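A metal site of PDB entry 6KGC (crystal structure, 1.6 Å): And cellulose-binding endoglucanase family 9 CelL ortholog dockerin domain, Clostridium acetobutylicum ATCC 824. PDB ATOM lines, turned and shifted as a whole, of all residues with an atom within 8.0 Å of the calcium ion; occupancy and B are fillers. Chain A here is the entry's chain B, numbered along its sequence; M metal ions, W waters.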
ATOM      1  N   ILE A   4      17.216   3.649   3.386  1.00  0.00           N
ATOM      2  CA  ILE A   4      17.294   2.773   4.550  1.00  0.00           C
ATOM      3  C   ILE A   4      18.735   2.608   5.016  1.00  0.00           C
ATOM      4  O   ILE A   4      19.579   2.122   4.265  1.00  0.00           O
ATOM      5  CB  ILE A   4      16.693   1.379   4.273  1.00  0.00           C
ATOM      6  CG1 ILE A   4      15.303   1.518   3.675  1.00  0.00           C
ATOM      7  CG2 ILE A   4      16.654   0.568   5.543  1.00  0.00           C
ATOM      8  CD1 ILE A   4      14.791   0.237   3.037  1.00  0.00           C
ATOM      9  N   GLY A   6      21.922   1.082   6.450  1.00  0.00           N
ATOM     10  CA  GLY A   6      22.357  -0.293   6.430  1.00  0.00           C
ATOM     11  C   GLY A   6      22.003  -1.050   5.166  1.00  0.00           C
ATOM     12  O   GLY A   6      22.553  -2.125   4.936  1.00  0.00           O
ATOM     13  N   ASP A   7      21.099  -0.524   4.328  1.00  0.00           N
ATOM     14  CA  ASP A   7      20.797  -1.147   3.039  1.00  0.00           C
ATOM     15  C   ASP A   7      21.774  -0.603   1.991  1.00  0.00           C
ATOM     16  O   ASP A   7      21.446   0.218   1.144  1.00  0.00           O
ATOM     17  CB  ASP A   7      19.353  -0.885   2.651  1.00  0.00           C
ATOM     18  CG  ASP A   7      18.948  -1.662   1.410  1.00  0.00           C
ATOM     19  OD1 ASP A   7      19.731  -2.549   0.999  1.00  0.00           O
ATOM     20  OD2 ASP A   7      17.857  -1.381   0.850  1.00  0.00           O
ATOM     21  N   LEU A   8      23.022  -1.084   2.092  1.00  0.00           N
ATOM     22  CA  LEU A   8      24.082  -0.548   1.247  1.00  0.00           C
ATOM     23  C   LEU A   8      23.866  -0.844  -0.234  1.00  0.00           C
ATOM     24  O   LEU A   8      24.364  -0.105  -1.091  1.00  0.00           O
ATOM     25  CB  LEU A   8      25.443  -1.102   1.700  1.00  0.00           C
ATOM     26  CG  LEU A   8      26.116  -0.431   2.892  1.00  0.00           C
ATOM     27  CD1 LEU A   8      25.221  -0.417   4.092  1.00  0.00           C
ATOM     28  CD2 LEU A   8      27.432  -1.144   3.242  1.00  0.00           C
ATOM     29  N   ASN A   9      23.155  -1.922  -0.570  1.00  0.00           N
ATOM     30  CA  ASN A   9      22.908  -2.244  -1.970  1.00  0.00           C
ATOM     31  C   ASN A   9      21.503  -1.860  -2.424  1.00  0.00           C
ATOM     32  O   ASN A   9      21.127  -2.184  -3.554  1.00  0.00           O
ATOM     33  CB  ASN A   9      23.122  -3.725  -2.246  1.00  0.00           C
ATOM     34  CG  ASN A   9      22.352  -4.623  -1.301  1.00  0.00           C
ATOM     35  OD1 ASN A   9      21.386  -4.219  -0.662  1.00  0.00           O
ATOM     36  ND2 ASN A   9      22.787  -5.882  -1.231  1.00  0.00           N
ATOM     37  N   ASP A  10      20.731  -1.195  -1.562  1.00  0.00           N
ATOM     38  CA  ASP A  10      19.425  -0.657  -1.921  1.00  0.00           C
ATOM     39  C   ASP A  10      18.517  -1.729  -2.508  1.00  0.00           C
ATOM     40  O   ASP A  10      17.698  -1.461  -3.387  1.00  0.00           O
ATOM     41  CB  ASP A  10      19.579   0.519  -2.891  1.00  0.00           C
ATOM     42  CG  ASP A  10      18.282   1.237  -3.161  1.00  0.00           C
ATOM     43  OD1 ASP A  10      17.348   1.103  -2.337  1.00  0.00           O
ATOM     44  OD2 ASP A  10      18.191   1.925  -4.191  1.00  0.00           O
ATOM     45  N   ASP A  11      18.651  -2.957  -2.020  1.00  0.00           N
ATOM     46  CA  ASP A  11      17.738  -4.020  -2.431  1.00  0.00           C
ATOM     47  C   ASP A  11      16.543  -4.173  -1.488  1.00  0.00           C
ATOM     48  O   ASP A  11      15.762  -5.105  -1.639  1.00  0.00           O
ATOM     49  CB  ASP A  11      18.484  -5.355  -2.604  1.00  0.00           C
ATOM     50  CG  ASP A  11      18.970  -5.963  -1.302  1.00  0.00           C
ATOM     51  OD1 ASP A  11      18.844  -5.326  -0.235  1.00  0.00           O
ATOM     52  OD2 ASP A  11      19.491  -7.097  -1.354  1.00  0.00           O
ATOM     53  N   GLY A  12      16.379  -3.252  -0.544  1.00  0.00           N
ATOM     54  CA  GLY A  12      15.196  -3.228   0.284  1.00  0.00           C
ATOM     55  C   GLY A  12      15.238  -4.092   1.526  1.00  0.00           C
ATOM     56  O   GLY A  12      14.245  -4.129   2.260  1.00  0.00           O
ATOM     57  N   VAL A  13      16.347  -4.786   1.771  1.00  0.00           N
ATOM     58  CA  VAL A  13      16.503  -5.540   3.007  1.00  0.00           C
ATOM     59  C   VAL A  13      17.911  -5.319   3.559  1.00  0.00           C
ATOM     60  O   VAL A  13      18.847  -4.978   2.831  1.00  0.00           O
ATOM     61  CB  VAL A  13      16.229  -7.054   2.844  1.00  0.00           C
ATOM     62  CG1 VAL A  13      14.806  -7.293   2.321  1.00  0.00           C
ATOM     63  CG2 VAL A  13      17.273  -7.715   1.950  1.00  0.00           C
ATOM     64  N   VAL A  14      18.022  -5.485   4.866  1.00  0.00           N
ATOM     65  CA  VAL A  14      19.297  -5.400   5.565  1.00  0.00           C
ATOM     66  C   VAL A  14      19.670  -6.817   5.964  1.00  0.00           C
ATOM     67  O   VAL A  14      19.006  -7.431   6.810  1.00  0.00           O
ATOM     68  CB  VAL A  14      19.213  -4.482   6.795  1.00  0.00           C
ATOM     69  CG1 VAL A  14      20.557  -4.363   7.461  1.00  0.00           C
ATOM     70  CG2 VAL A  14      18.698  -3.112   6.385  1.00  0.00           C
ATOM     71  N   ASN A  15      20.686  -7.360   5.306  1.00  0.00           N
ATOM     72  CA  ASN A  15      21.117  -8.737   5.551  1.00  0.00           C
ATOM     73  C   ASN A  15      22.617  -8.833   5.338  1.00  0.00           C
ATOM     74  O   ASN A  15      23.329  -7.828   5.243  1.00  0.00           O
ATOM     75  CB  ASN A  15      20.347  -9.718   4.677  1.00  0.00           C
ATOM     76  CG  ASN A  15      20.575  -9.512   3.184  1.00  0.00           C
ATOM     77  OD1 ASN A  15      21.495  -8.817   2.770  1.00  0.00           O
ATOM     78  ND2 ASN A  15      19.732 -10.152   2.374  1.00  0.00           N
ATOM     79  N   GLY A  16      23.102 -10.070   5.262  1.00  0.00           N
ATOM     80  CA  GLY A  16      24.522 -10.307   5.188  1.00  0.00           C
ATOM     81  C   GLY A  16      25.200  -9.699   3.972  1.00  0.00           C
ATOM     82  O   GLY A  16      26.399  -9.418   4.019  1.00  0.00           O
ATOM     83  N   ARG A  17      24.468  -9.547   2.860  1.00  0.00           N
ATOM     84  CA  ARG A  17      25.090  -8.913   1.696  1.00  0.00           C
ATOM     85  C   ARG A  17      25.545  -7.492   2.036  1.00  0.00           C
ATOM     86  O   ARG A  17      26.562  -7.010   1.514  1.00  0.00           O
ATOM     87  CB  ARG A  17      24.125  -8.858   0.534  1.00  0.00           C
ATOM     88  CG  ARG A  17      23.701 -10.193  -0.041  1.00  0.00           C
ATOM     89  CD  ARG A  17      22.961  -9.907  -1.314  1.00  0.00           C
ATOM     90  NE  ARG A  17      22.121 -10.950  -1.864  1.00  0.00           N
ATOM     91  CZ  ARG A  17      22.537 -11.931  -2.654  1.00  0.00           C
ATOM     92  NH1 ARG A  17      23.839 -12.065  -2.901  1.00  0.00           N
ATOM     93  NH2 ARG A  17      21.671 -12.807  -3.143  1.00  0.00           N
ATOM     94  N   ASP A  18      24.765  -6.809   2.872  1.00  0.00           N
ATOM     95  CA  ASP A  18      25.102  -5.445   3.278  1.00  0.00           C
ATOM     96  C   ASP A  18      26.314  -5.439   4.206  1.00  0.00           C
ATOM     97  O   ASP A  18      27.157  -4.541   4.130  1.00  0.00           O
ATOM     98  CB  ASP A  18      23.897  -4.813   3.962  1.00  0.00           C
ATOM     99  CG  ASP A  18      22.681  -4.727   3.060  1.00  0.00           C
ATOM    100  OD1 ASP A  18      22.737  -4.009   2.058  1.00  0.00           O
ATOM    101  OD2 ASP A  18      21.676  -5.389   3.367  1.00  0.00           O
ATOM    102  N   ILE A  19      26.425  -6.441   5.071  1.00  0.00           N
ATOM    103  CA  ILE A  19      27.607  -6.548   5.913  1.00  0.00           C
ATOM    104  C   ILE A  19      28.853  -6.683   5.060  1.00  0.00           C
ATOM    105  O   ILE A  19      29.888  -6.047   5.306  1.00  0.00           O
ATOM    106  CB  ILE A  19      27.457  -7.738   6.880  1.00  0.00           C
ATOM    107  CG1 ILE A  19      26.433  -7.412   7.942  1.00  0.00           C
ATOM    108  CG2 ILE A  19      28.790  -8.081   7.553  1.00  0.00           C
ATOM    109  CD1 ILE A  19      26.076  -8.581   8.793  1.00  0.00           C
ATOM    110  N   MET A  21      29.386  -5.670   2.040  1.00  0.00           N
ATOM    111  CA  MET A  21      29.665  -4.399   1.387  1.00  0.00           C
ATOM    112  C   MET A  21      30.266  -3.380   2.349  1.00  0.00           C
ATOM    113  O   MET A  21      31.164  -2.631   1.966  1.00  0.00           O
ATOM    114  CB  MET A  21      28.368  -3.851   0.763  1.00  0.00           C
ATOM    115  CG  MET A  21      27.936  -4.629  -0.434  1.00  0.00           C
ATOM    116  SD  MET A  21      26.410  -3.984  -1.138  1.00  0.00           S
ATOM    117  CE  MET A  21      26.852  -2.300  -1.427  1.00  0.00           C
ATOM    118  N   LEU A  55      25.381  -2.152  12.033  1.00  0.00           N
ATOM    119  CA  LEU A  55      24.799  -2.966  10.980  1.00  0.00           C
ATOM    120  C   LEU A  55      24.673  -4.415  11.432  1.00  0.00           C
ATOM    121  O   LEU A  55      23.651  -5.071  11.192  1.00  0.00           O
ATOM    122  CB  LEU A  55      25.658  -2.852   9.723  1.00  0.00           C
ATOM    123  CG  LEU A  55      25.209  -3.629   8.498  1.00  0.00           C
ATOM    124  CD1 LEU A  55      23.810  -3.262   8.060  1.00  0.00           C
ATOM    125  CD2 LEU A  55      26.223  -3.393   7.355  1.00  0.00           C
HETATM  126 CA    CA M   1      20.477  -4.753   1.307  1.00  0.00          CA
HETATM  127  O   HOH W   1      21.053  -7.015   0.932  1.00  0.00           O
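The backbone NH of Asp 10 lies close to the side-chain carboxylate of Asp 7, 3.1 Å away. N of Gly 12 lies within hydrogen-bond range of OD2 of Asp 7, 2.8 Å away. The backbone NH (N) of Asn 15 lies close to the side-chain carboxylate (OD2) of Asp 18 (2.9 Å). The side-chain carboxylate (OD1) of Asp 18 sits close to the backbone NH (N) of Leu 8, at 2.9 Å.
Water W1 lies within hydrogen-bond range of OD1 of Asn 15, OD2 of Asp 11 and ND2 of Asn 9.
Within 4 Å of the calcium ion: Asp 7, Asn 9, Asp 11, Val 13 and Asp 18. The nearest printed residue that does not touch the calcium ion is Val 14 (4.4 Å).
The calcium ion is bound by OD1 of Asn 9 (2.2 Å), O of Val 13 (2.2 Å), OD1 of Asp 11 (2.3 Å), OD1 of Asp 7 (2.3 Å), water W1 (2.4 Å), OD2 of Asp 18 (2.5 Å) and OD1 of Asp 18 (2.5 Å). The calcium ion has seven donor atoms within binding distance.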
